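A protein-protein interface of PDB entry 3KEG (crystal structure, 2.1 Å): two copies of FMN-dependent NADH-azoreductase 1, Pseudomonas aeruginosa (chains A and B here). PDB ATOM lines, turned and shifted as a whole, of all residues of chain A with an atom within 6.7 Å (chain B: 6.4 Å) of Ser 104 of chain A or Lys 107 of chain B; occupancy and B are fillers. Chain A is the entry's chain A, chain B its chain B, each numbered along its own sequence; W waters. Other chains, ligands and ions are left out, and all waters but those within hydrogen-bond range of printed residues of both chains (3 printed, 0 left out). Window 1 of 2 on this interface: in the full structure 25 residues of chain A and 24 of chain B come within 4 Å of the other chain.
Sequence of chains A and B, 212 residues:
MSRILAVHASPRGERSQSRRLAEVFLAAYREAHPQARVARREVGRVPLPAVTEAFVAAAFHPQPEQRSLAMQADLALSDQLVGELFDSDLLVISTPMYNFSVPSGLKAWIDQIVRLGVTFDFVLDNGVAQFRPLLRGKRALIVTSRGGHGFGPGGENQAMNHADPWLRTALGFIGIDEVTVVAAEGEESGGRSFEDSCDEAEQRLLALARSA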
ATOM      1  N   ALA A   9      25.013   7.398 -19.381  1.00  0.00           N
ATOM      2  CA  ALA A   9      24.823   7.785 -17.981  1.00  0.00           C
ATOM      3  C   ALA A   9      26.116   8.070 -17.213  1.00  0.00           C
ATOM      4  O   ALA A   9      26.075   8.663 -16.136  1.00  0.00           O
ATOM      5  CB  ALA A   9      24.009   6.723 -17.249  1.00  0.00           C
ATOM      6  N   VAL A  43      22.887  11.955 -20.202  1.00  0.00           N
ATOM      7  CA  VAL A  43      22.366  12.132 -18.852  1.00  0.00           C
ATOM      8  C   VAL A  43      23.460  11.970 -17.793  1.00  0.00           C
ATOM      9  O   VAL A  43      23.180  11.996 -16.596  1.00  0.00           O
ATOM     10  CB  VAL A  43      21.203  11.155 -18.563  1.00  0.00           C
ATOM     11  CG1 VAL A  43      20.150  11.256 -19.655  1.00  0.00           C
ATOM     12  CG2 VAL A  43      21.707   9.723 -18.441  1.00  0.00           C
ATOM     13  N   LEU A  48      20.497  16.554 -15.486  1.00  0.00           N
ATOM     14  CA  LEU A  48      19.072  16.409 -15.743  1.00  0.00           C
ATOM     15  C   LEU A  48      18.308  16.863 -14.508  1.00  0.00           C
ATOM     16  O   LEU A  48      18.601  16.419 -13.399  1.00  0.00           O
ATOM     17  CB  LEU A  48      18.714  14.959 -16.057  1.00  0.00           C
ATOM     18  CG  LEU A  48      18.396  14.652 -17.518  1.00  0.00           C
ATOM     19  CD1 LEU A  48      19.674  14.498 -18.324  1.00  0.00           C
ATOM     20  CD2 LEU A  48      17.543  13.399 -17.604  1.00  0.00           C
ATOM     21  N   MET A  97      27.890   1.244 -12.406  1.00  0.00           N
ATOM     22  CA  MET A  97      27.222   1.001 -11.139  1.00  0.00           C
ATOM     23  C   MET A  97      27.797   1.973 -10.122  1.00  0.00           C
ATOM     24  O   MET A  97      28.986   1.926  -9.806  1.00  0.00           O
ATOM     25  CB  MET A  97      27.413  -0.435 -10.655  1.00  0.00           C
ATOM     26  CG  MET A  97      26.996  -0.621  -9.203  1.00  0.00           C
ATOM     27  SD  MET A  97      27.155  -2.314  -8.608  1.00  0.00           S
ATOM     28  CE  MET A  97      25.691  -3.068  -9.311  1.00  0.00           C
ATOM     29  N   TYR A  98      26.952   2.872  -9.634  1.00  0.00           N
ATOM     30  CA  TYR A  98      27.342   3.818  -8.599  1.00  0.00           C
ATOM     31  C   TYR A  98      26.646   3.460  -7.294  1.00  0.00           C
ATOM     32  O   TYR A  98      25.428   3.578  -7.177  1.00  0.00           O
ATOM     33  CB  TYR A  98      26.970   5.242  -9.007  1.00  0.00           C
ATOM     34  CG  TYR A  98      28.003   5.958  -9.852  1.00  0.00           C
ATOM     35  CD1 TYR A  98      29.069   5.275 -10.428  1.00  0.00           C
ATOM     36  CD2 TYR A  98      27.904   7.325 -10.075  1.00  0.00           C
ATOM     37  CE1 TYR A  98      30.008   5.938 -11.199  1.00  0.00           C
ATOM     38  CE2 TYR A  98      28.835   7.995 -10.844  1.00  0.00           C
ATOM     39  CZ  TYR A  98      29.884   7.298 -11.402  1.00  0.00           C
ATOM     40  OH  TYR A  98      30.810   7.961 -12.169  1.00  0.00           O
ATOM     41  N   ASN A  99      27.433   3.025  -6.317  1.00  0.00           N
ATOM     42  CA  ASN A  99      26.913   2.645  -5.011  1.00  0.00           C
ATOM     43  C   ASN A  99      25.700   1.726  -5.131  1.00  0.00           C
ATOM     44  O   ASN A  99      24.644   1.987  -4.560  1.00  0.00           O
ATOM     45  CB  ASN A  99      26.612   3.902  -4.190  1.00  0.00           C
ATOM     46  CG  ASN A  99      27.866   4.705  -3.891  1.00  0.00           C
ATOM     47  OD1 ASN A  99      28.795   4.206  -3.262  1.00  0.00           O
ATOM     48  ND2 ASN A  99      27.904   5.945  -4.360  1.00  0.00           N
ATOM     49  N   PHE A 100      25.881   0.650  -5.893  1.00  0.00           N
ATOM     50  CA  PHE A 100      24.902  -0.430  -6.020  1.00  0.00           C
ATOM     51  C   PHE A 100      23.615  -0.012  -6.730  1.00  0.00           C
ATOM     52  O   PHE A 100      22.608  -0.714  -6.669  1.00  0.00           O
ATOM     53  CB  PHE A 100      24.594  -1.023  -4.645  1.00  0.00           C
ATOM     54  CG  PHE A 100      25.822  -1.303  -3.832  1.00  0.00           C
ATOM     55  CD1 PHE A 100      26.649  -2.366  -4.151  1.00  0.00           C
ATOM     56  CD2 PHE A 100      26.159  -0.495  -2.759  1.00  0.00           C
ATOM     57  CE1 PHE A 100      27.785  -2.625  -3.412  1.00  0.00           C
ATOM     58  CE2 PHE A 100      27.294  -0.748  -2.015  1.00  0.00           C
ATOM     59  CZ  PHE A 100      28.109  -1.815  -2.342  1.00  0.00           C
ATOM     60  N   SER A 101      23.660   1.130  -7.406  1.00  0.00           N
ATOM     61  CA  SER A 101      22.560   1.567  -8.257  1.00  0.00           C
ATOM     62  C   SER A 101      23.145   2.281  -9.476  1.00  0.00           C
ATOM     63  O   SER A 101      24.277   2.007  -9.870  1.00  0.00           O
ATOM     64  CB  SER A 101      21.605   2.475  -7.477  1.00  0.00           C
ATOM     65  OG  SER A 101      20.431   2.751  -8.221  1.00  0.00           O
ATOM     66  N   VAL A 102      22.379   3.185 -10.079  1.00  0.00           N
ATOM     67  CA  VAL A 102      22.856   3.956 -11.225  1.00  0.00           C
ATOM     68  C   VAL A 102      23.175   5.385 -10.812  1.00  0.00           C
ATOM     69  O   VAL A 102      22.670   5.864  -9.798  1.00  0.00           O
ATOM     70  CB  VAL A 102      21.801   4.013 -12.342  1.00  0.00           C
ATOM     71  CG1 VAL A 102      21.513   2.621 -12.877  1.00  0.00           C
ATOM     72  CG2 VAL A 102      20.522   4.673 -11.835  1.00  0.00           C
ATOM     73  N   PRO A 103      24.010   6.077 -11.602  1.00  0.00           N
ATOM     74  CA  PRO A 103      24.248   7.496 -11.322  1.00  0.00           C
ATOM     75  C   PRO A 103      22.921   8.245 -11.228  1.00  0.00           C
ATOM     76  O   PRO A 103      21.952   7.843 -11.870  1.00  0.00           O
ATOM     77  CB  PRO A 103      25.061   7.964 -12.533  1.00  0.00           C
ATOM     78  CG  PRO A 103      25.719   6.729 -13.048  1.00  0.00           C
ATOM     79  CD  PRO A 103      24.753   5.612 -12.786  1.00  0.00           C
ATOM     80  N   SER A 104      22.878   9.312 -10.437  1.00  0.00           N
ATOM     81  CA  SER A 104      21.624  10.004 -10.158  1.00  0.00           C
ATOM     82  C   SER A 104      20.998  10.610 -11.413  1.00  0.00           C
ATOM     83  O   SER A 104      19.784  10.792 -11.479  1.00  0.00           O
ATOM     84  CB  SER A 104      21.836  11.089  -9.099  1.00  0.00           C
ATOM     85  OG  SER A 104      22.736  12.088  -9.549  1.00  0.00           O
ATOM     86  N   GLY A 105      21.827  10.921 -12.402  1.00  0.00           N
ATOM     87  CA  GLY A 105      21.346  11.482 -13.652  1.00  0.00           C
ATOM     88  C   GLY A 105      20.451  10.522 -14.417  1.00  0.00           C
ATOM     89  O   GLY A 105      19.481  10.939 -15.050  1.00  0.00           O
ATOM     90  N   LEU A 106      20.774   9.233 -14.365  1.00  0.00           N
ATOM     91  CA  LEU A 106      19.967   8.221 -15.042  1.00  0.00           C
ATOM     92  C   LEU A 106      18.660   7.979 -14.293  1.00  0.00           C
ATOM     93  O   LEU A 106      17.623   7.736 -14.908  1.00  0.00           O
ATOM     94  CB  LEU A 106      20.745   6.910 -15.189  1.00  0.00           C
ATOM     95  CG  LEU A 106      19.986   5.755 -15.853  1.00  0.00           C
ATOM     96  CD1 LEU A 106      19.379   6.183 -17.181  1.00  0.00           C
ATOM     97  CD2 LEU A 106      20.900   4.557 -16.046  1.00  0.00           C
ATOM     98  N   LYS A 107      18.708   8.036 -12.966  1.00  0.00           N
ATOM     99  CA  LYS A 107      17.487   7.954 -12.173  1.00  0.00           C
ATOM    100  C   LYS A 107      16.557   9.091 -12.570  1.00  0.00           C
ATOM    101  O   LYS A 107      15.351   8.901 -12.708  1.00  0.00           O
ATOM    102  CB  LYS A 107      17.788   8.032 -10.675  1.00  0.00           C
ATOM    103  CG  LYS A 107      16.536   8.036  -9.792  1.00  0.00           C
ATOM    104  CD  LYS A 107      15.963   6.634  -9.621  1.00  0.00           C
ATOM    105  CE  LYS A 107      14.502   6.547 -10.048  1.00  0.00           C
ATOM    106  NZ  LYS A 107      13.574   7.260  -9.125  1.00  0.00           N
ATOM    107  N   ALA A 108      17.129  10.277 -12.751  1.00  0.00           N
ATOM    108  CA  ALA A 108      16.355  11.451 -13.131  1.00  0.00           C
ATOM    109  C   ALA A 108      15.757  11.294 -14.531  1.00  0.00           C
ATOM    110  O   ALA A 108      14.636  11.735 -14.783  1.00  0.00           O
ATOM    111  CB  ALA A 108      17.218  12.706 -13.051  1.00  0.00           C
ATOM    112  N   TRP A 109      16.500  10.665 -15.438  1.00  0.00           N
ATOM    113  CA  TRP A 109      15.983  10.399 -16.778  1.00  0.00           C
ATOM    114  C   TRP A 109      14.741   9.519 -16.695  1.00  0.00           C
ATOM    115  O   TRP A 109      13.707   9.838 -17.280  1.00  0.00           O
ATOM    116  CB  TRP A 109      17.036   9.727 -17.666  1.00  0.00           C
ATOM    117  CG  TRP A 109      16.549   9.487 -19.069  1.00  0.00           C
ATOM    118  CD1 TRP A 109      16.412  10.417 -20.056  1.00  0.00           C
ATOM    119  CD2 TRP A 109      16.133   8.232 -19.637  1.00  0.00           C
ATOM    120  NE1 TRP A 109      15.936   9.825 -21.202  1.00  0.00           N
ATOM    121  CE2 TRP A 109      15.759   8.493 -20.973  1.00  0.00           C
ATOM    122  CE3 TRP A 109      16.043   6.928 -19.147  1.00  0.00           C
ATOM    123  CZ2 TRP A 109      15.300   7.483 -21.823  1.00  0.00           C
ATOM    124  CZ3 TRP A 109      15.586   5.930 -19.996  1.00  0.00           C
ATOM    125  CH2 TRP A 109      15.221   6.214 -21.319  1.00  0.00           C
ATOM    126  N   LEU B  48      20.615  18.677  -5.734  1.00  0.00           N
ATOM    127  CA  LEU B  48      21.891  18.232  -5.205  1.00  0.00           C
ATOM    128  C   LEU B  48      22.746  17.773  -6.377  1.00  0.00           C
ATOM    129  O   LEU B  48      22.366  16.853  -7.101  1.00  0.00           O
ATOM    130  CB  LEU B  48      21.684  17.086  -4.214  1.00  0.00           C
ATOM    131  CG  LEU B  48      22.665  17.016  -3.044  1.00  0.00           C
ATOM    132  CD1 LEU B  48      22.488  18.218  -2.125  1.00  0.00           C
ATOM    133  CD2 LEU B  48      22.467  15.721  -2.275  1.00  0.00           C
ATOM    134  N   PRO B  49      23.902  18.423  -6.581  1.00  0.00           N
ATOM    135  CA  PRO B  49      24.749  18.100  -7.732  1.00  0.00           C
ATOM    136  C   PRO B  49      25.003  16.606  -7.880  1.00  0.00           C
ATOM    137  O   PRO B  49      25.211  15.908  -6.888  1.00  0.00           O
ATOM    138  CB  PRO B  49      26.065  18.828  -7.422  1.00  0.00           C
ATOM    139  CG  PRO B  49      25.956  19.266  -5.983  1.00  0.00           C
ATOM    140  CD  PRO B  49      24.503  19.486  -5.761  1.00  0.00           C
ATOM    141  N   ALA B  50      24.980  16.127  -9.118  1.00  0.00           N
ATOM    142  CA  ALA B  50      25.330  14.747  -9.409  1.00  0.00           C
ATOM    143  C   ALA B  50      26.844  14.608  -9.395  1.00  0.00           C
ATOM    144  O   ALA B  50      27.567  15.591  -9.560  1.00  0.00           O
ATOM    145  CB  ALA B  50      24.781  14.342 -10.761  1.00  0.00           C
ATOM    146  N   VAL B  51      27.323  13.387  -9.191  1.00  0.00           N
ATOM    147  CA  VAL B  51      28.748  13.111  -9.269  1.00  0.00           C
ATOM    148  C   VAL B  51      29.255  13.397 -10.679  1.00  0.00           C
ATOM    149  O   VAL B  51      28.724  12.872 -11.657  1.00  0.00           O
ATOM    150  CB  VAL B  51      29.053  11.648  -8.899  1.00  0.00           C
ATOM    151  CG1 VAL B  51      30.406  11.220  -9.447  1.00  0.00           C
ATOM    152  CG2 VAL B  51      28.991  11.461  -7.389  1.00  0.00           C
ATOM    153  N   SER B 101      12.335   3.118  -7.093  1.00  0.00           N
ATOM    154  CA  SER B 101      13.582   3.493  -6.433  1.00  0.00           C
ATOM    155  C   SER B 101      13.341   4.773  -5.630  1.00  0.00           C
ATOM    156  O   SER B 101      12.212   5.045  -5.228  1.00  0.00           O
ATOM    157  CB  SER B 101      14.699   3.679  -7.465  1.00  0.00           C
ATOM    158  OG  SER B 101      15.957   3.867  -6.842  1.00  0.00           O
ATOM    159  N   VAL B 102      14.392   5.549  -5.386  1.00  0.00           N
ATOM    160  CA  VAL B 102      14.260   6.811  -4.666  1.00  0.00           C
ATOM    161  C   VAL B 102      14.387   7.984  -5.629  1.00  0.00           C
ATOM    162  O   VAL B 102      14.939   7.835  -6.718  1.00  0.00           O
ATOM    163  CB  VAL B 102      15.345   6.960  -3.582  1.00  0.00           C
ATOM    164  CG1 VAL B 102      15.277   5.806  -2.597  1.00  0.00           C
ATOM    165  CG2 VAL B 102      16.730   7.043  -4.217  1.00  0.00           C
ATOM    166  N   PRO B 103      13.873   9.158  -5.233  1.00  0.00           N
ATOM    167  CA  PRO B 103      14.079  10.359  -6.045  1.00  0.00           C
ATOM    168  C   PRO B 103      15.563  10.563  -6.340  1.00  0.00           C
ATOM    169  O   PRO B 103      16.399  10.205  -5.513  1.00  0.00           O
ATOM    170  CB  PRO B 103      13.535  11.477  -5.151  1.00  0.00           C
ATOM    171  CG  PRO B 103      12.501  10.807  -4.318  1.00  0.00           C
ATOM    172  CD  PRO B 103      13.041   9.430  -4.048  1.00  0.00           C
ATOM    173  N   SER B 104      15.882  11.120  -7.503  1.00  0.00           N
ATOM    174  CA  SER B 104      17.273  11.232  -7.938  1.00  0.00           C
ATOM    175  C   SER B 104      18.116  12.061  -6.974  1.00  0.00           C
ATOM    176  O   SER B 104      19.327  11.872  -6.880  1.00  0.00           O
ATOM    177  CB  SER B 104      17.352  11.825  -9.348  1.00  0.00           C
ATOM    178  OG  SER B 104      16.764  13.112  -9.405  1.00  0.00           O
ATOM    179  N   GLY B 105      17.474  12.983  -6.266  1.00  0.00           N
ATOM    180  CA  GLY B 105      18.159  13.806  -5.287  1.00  0.00           C
ATOM    181  C   GLY B 105      18.774  12.994  -4.161  1.00  0.00           C
ATOM    182  O   GLY B 105      19.865  13.311  -3.688  1.00  0.00           O
ATOM    183  N   LEU B 106      18.075  11.950  -3.724  1.00  0.00           N
ATOM    184  CA  LEU B 106      18.577  11.096  -2.650  1.00  0.00           C
ATOM    185  C   LEU B 106      19.678  10.167  -3.159  1.00  0.00           C
ATOM    186  O   LEU B 106      20.595   9.820  -2.416  1.00  0.00           O
ATOM    187  CB  LEU B 106      17.440  10.285  -2.019  1.00  0.00           C
ATOM    188  CG  LEU B 106      17.825   9.403  -0.825  1.00  0.00           C
ATOM    189  CD1 LEU B 106      18.472  10.222   0.284  1.00  0.00           C
ATOM    190  CD2 LEU B 106      16.610   8.658  -0.289  1.00  0.00           C
ATOM    191  N   LYS B 107      19.586   9.760  -4.422  1.00  0.00           N
ATOM    192  CA  LYS B 107      20.658   8.987  -5.039  1.00  0.00           C
ATOM    193  C   LYS B 107      21.920   9.837  -5.102  1.00  0.00           C
ATOM    194  O   LYS B 107      23.023   9.347  -4.872  1.00  0.00           O
ATOM    195  CB  LYS B 107      20.274   8.529  -6.449  1.00  0.00           C
ATOM    196  CG  LYS B 107      21.375   7.744  -7.172  1.00  0.00           C
ATOM    197  CD  LYS B 107      21.457   6.300  -6.682  1.00  0.00           C
ATOM    198  CE  LYS B 107      22.860   5.907  -6.218  1.00  0.00           C
ATOM    199  NZ  LYS B 107      23.901   5.970  -7.283  1.00  0.00           N
ATOM    200  N   ALA B 108      21.747  11.117  -5.415  1.00  0.00           N
ATOM    201  CA  ALA B 108      22.865  12.049  -5.493  1.00  0.00           C
ATOM    202  C   ALA B 108      23.502  12.256  -4.120  1.00  0.00           C
ATOM    203  O   ALA B 108      24.723  12.359  -4.007  1.00  0.00           O
ATOM    204  CB  ALA B 108      22.406  13.381  -6.073  1.00  0.00           C
ATOM    205  N   TRP B 109      22.676  12.314  -3.079  1.00  0.00           N
ATOM    206  CA  TRP B 109      23.181  12.479  -1.720  1.00  0.00           C
ATOM    207  C   TRP B 109      24.059  11.293  -1.341  1.00  0.00           C
ATOM    208  O   TRP B 109      25.160  11.464  -0.820  1.00  0.00           O
ATOM    209  CB  TRP B 109      22.032  12.621  -0.718  1.00  0.00           C
ATOM    210  CG  TRP B 109      22.505  12.816   0.691  1.00  0.00           C
ATOM    211  CD1 TRP B 109      23.002  13.964   1.233  1.00  0.00           C
ATOM    212  CD2 TRP B 109      22.525  11.832   1.739  1.00  0.00           C
ATOM    213  NE1 TRP B 109      23.333  13.758   2.551  1.00  0.00           N
ATOM    214  CE2 TRP B 109      23.051  12.466   2.885  1.00  0.00           C
ATOM    215  CE3 TRP B 109      22.152  10.489   1.815  1.00  0.00           C
ATOM    216  CZ2 TRP B 109      23.210  11.791   4.097  1.00  0.00           C
ATOM    217  CZ3 TRP B 109      22.312   9.824   3.021  1.00  0.00           C
ATOM    218  CH2 TRP B 109      22.837  10.477   4.146  1.00  0.00           C
ATOM    219  N   ILE B 110      23.563  10.090  -1.608  1.00  0.00           N
ATOM    220  CA  ILE B 110      24.323   8.875  -1.344  1.00  0.00           C
ATOM    221  C   ILE B 110      25.664   8.916  -2.072  1.00  0.00           C
ATOM    222  O   ILE B 110      26.705   8.604  -1.494  1.00  0.00           O
ATOM    223  CB  ILE B 110      23.538   7.617  -1.777  1.00  0.00           C
ATOM    224  CG1 ILE B 110      22.414   7.317  -0.779  1.00  0.00           C
ATOM    225  CG2 ILE B 110      24.466   6.415  -1.886  1.00  0.00           C
ATOM    226  CD1 ILE B 110      22.901   6.929   0.603  1.00  0.00           C
ATOM    227  N   ASP B 111      25.631   9.308  -3.341  1.00  0.00           N
ATOM    228  CA  ASP B 111      26.837   9.366  -4.161  1.00  0.00           C
ATOM    229  C   ASP B 111      27.864  10.372  -3.637  1.00  0.00           C
ATOM    230  O   ASP B 111      29.058  10.232  -3.902  1.00  0.00           O
ATOM    231  CB  ASP B 111      26.477   9.696  -5.616  1.00  0.00           C
ATOM    232  CG  ASP B 111      25.832   8.527  -6.347  1.00  0.00           C
ATOM    233  OD1 ASP B 111      25.881   7.396  -5.829  1.00  0.00           O
ATOM    234  OD2 ASP B 111      25.280   8.749  -7.443  1.00  0.00           O
ATOM    235  N   GLN B 112      27.405  11.386  -2.906  1.00  0.00           N
ATOM    236  CA  GLN B 112      28.319  12.377  -2.327  1.00  0.00           C
ATOM    237  C   GLN B 112      28.980  11.887  -1.042  1.00  0.00           C
ATOM    238  O   GLN B 112      30.113  12.264  -0.741  1.00  0.00           O
ATOM    239  CB  GLN B 112      27.598  13.701  -2.039  1.00  0.00           C
ATOM    240  CG  GLN B 112      27.236  14.510  -3.275  1.00  0.00           C
ATOM    241  CD  GLN B 112      28.457  15.080  -3.978  1.00  0.00           C
ATOM    242  OE1 GLN B 112      29.299  15.733  -3.361  1.00  0.00           O
ATOM    243  NE2 GLN B 112      28.554  14.841  -5.281  1.00  0.00           N
ATOM    244  N   TRP B 166      17.555  -0.996  -1.332  1.00  0.00           N
ATOM    245  CA  TRP B 166      18.812  -0.512  -1.884  1.00  0.00           C
ATOM    246  C   TRP B 166      19.509   0.433  -0.908  1.00  0.00           C
ATOM    247  O   TRP B 166      20.735   0.432  -0.804  1.00  0.00           O
ATOM    248  CB  TRP B 166      18.610   0.202  -3.217  1.00  0.00           C
ATOM    249  CG  TRP B 166      19.772   1.077  -3.527  1.00  0.00           C
ATOM    250  CD1 TRP B 166      20.979   0.685  -4.022  1.00  0.00           C
ATOM    251  CD2 TRP B 166      19.861   2.493  -3.318  1.00  0.00           C
ATOM    252  NE1 TRP B 166      21.809   1.771  -4.152  1.00  0.00           N
ATOM    253  CE2 TRP B 166      21.149   2.888  -3.729  1.00  0.00           C
ATOM    254  CE3 TRP B 166      18.975   3.458  -2.836  1.00  0.00           C
ATOM    255  CZ2 TRP B 166      21.570   4.215  -3.669  1.00  0.00           C
ATOM    256  CZ3 TRP B 166      19.397   4.773  -2.779  1.00  0.00           C
ATOM    257  CH2 TRP B 166      20.683   5.140  -3.194  1.00  0.00           C
HETATM  258  O   HOH W   1      30.454   7.881  -3.996  1.00  0.00           O
HETATM  259  O   HOH W   2      18.090   1.886  -7.403  1.00  0.00           O
HETATM  260  O   HOH W   3      25.196  10.829  -8.964  1.00  0.00           O
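The backbone carbonyl oxygen (O) of Tyr 98 of chain A sits at hydrogen-bond distance from the side-chain amino group (NZ) of Lys 107 of chain B, 2.8 Å away.
ND2 of Asn 99 of chain A lies within hydrogen-bond range of OD1 of Asp 111 of chain B, at 2.9 Å.
The indole nitrogen (NE1) of Trp 166 of chain B lies within hydrogen-bond range of the backbone carbonyl oxygen (O) of Asn 99 of chain A (2.9 Å).
The side-chain amino group (NZ) of Lys 107 of chain B is in hydrogen-bond range of the backbone carbonyl oxygen (O) of Val 102 of chain A (2.8 Å).
O of Val 102 of chain B is in hydrogen-bond range of NZ of Lys 107 of chain A.
NZ of Lys 107 of chain B lies within salt-bridge range of OD1 of Asp 111 of chain B (2.8 Å).
Among the printed residues, pairs that only touch across the chains: Ser 104 of chain A with Ala 50 of chain B, Ser 104 of chain A with Ser 104 of chain B, Ser 101 of chain A with Trp 166 of chain B, Phe 100 of chain A with Trp 166 of chain B, Ser 104 of chain A with Ala 108 of chain B, Ala 108 of chain A with Ser 104 of chain B, Ser 104 of chain A with Lys 107 of chain B, Lys 107 of chain A with Ser 104 of chain B, Tyr 98 of chain A with Val 51 of chain B, Lys 107 of chain A with Ser 101 of chain B, Ser 101 of chain A with Lys 107 of chain B, Ser 104 of chain A with Asp 111 of chain B and Tyr 98 of chain A with Asp 111 of chain B.
Of the printed residues of chain B, Ser 104 of chain A touches Ala 50, Ser 104, Lys 107, Ala 108 and Asp 111.
Of the printed residues of chain B, Ala 108 of chain A touches Ser 104.
Of the printed residues of chain A, Ala 50 of chain B touches Ser 104.
Of the printed residues of chain A, Val 51 of chain B touches Tyr 98 (3.8 Å).
Printed residues of chain B within 4 Å of Ser 101 of chain A: Lys 107 and Trp 166.
Trp 109 of chain A touches none of the printed residues of chain B.
The nearest residue of chain A that does not touch Lys 107 of chain B is Pro 103 of chain A (4.3 Å).
Of the 17 printed residues of chain B, 9 touch a printed residue of chain A.
Hydrophobic or aromatic side chains of chain B within 4 Å of the printed part of chain A: Ala 50, Val 51, Ala 108 and Trp 166.
Among the printed residues, no Asp or Glu carboxylate lies within 4 Å of a Lys or Arg side-chain nitrogen of the other chain.
Ser 101 of chain A touches Lys 107 of chain B, and with the chains exchanged Lys 107 of chain A touches Ser 101 of chain B.
Val 102 of chain A touches Lys 107 of chain B, and with the chains exchanged Lys 107 of chain A touches Val 102 of chain B.
Ser 104 of chain A touches Lys 107 of chain B, and with the chains exchanged Lys 107 of chain A touches Ser 104 of chain B.
Ser 104 of chain A touches Ala 108 of chain B, and with the chains exchanged Ala 108 of chain A touches Ser 104 of chain B.
Water W3 lies within hydrogen-bond range of OD2 of Asp 111 of chain B, OG of Ser 104 of chain A and N of Val 51 of chain B.
Water W2 bridges the side-chain hydroxyl of Ser 101 of chain A (2.6 Å) and the side-chain hydroxyl of Ser 101 of chain B (3.0 Å).
Water W1 bridges the backbone carbonyl oxygen of Asp 111 of chain B (2.7 Å) and the side-chain amide nitrogen of Asn 99 of chain A (3.2 Å).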
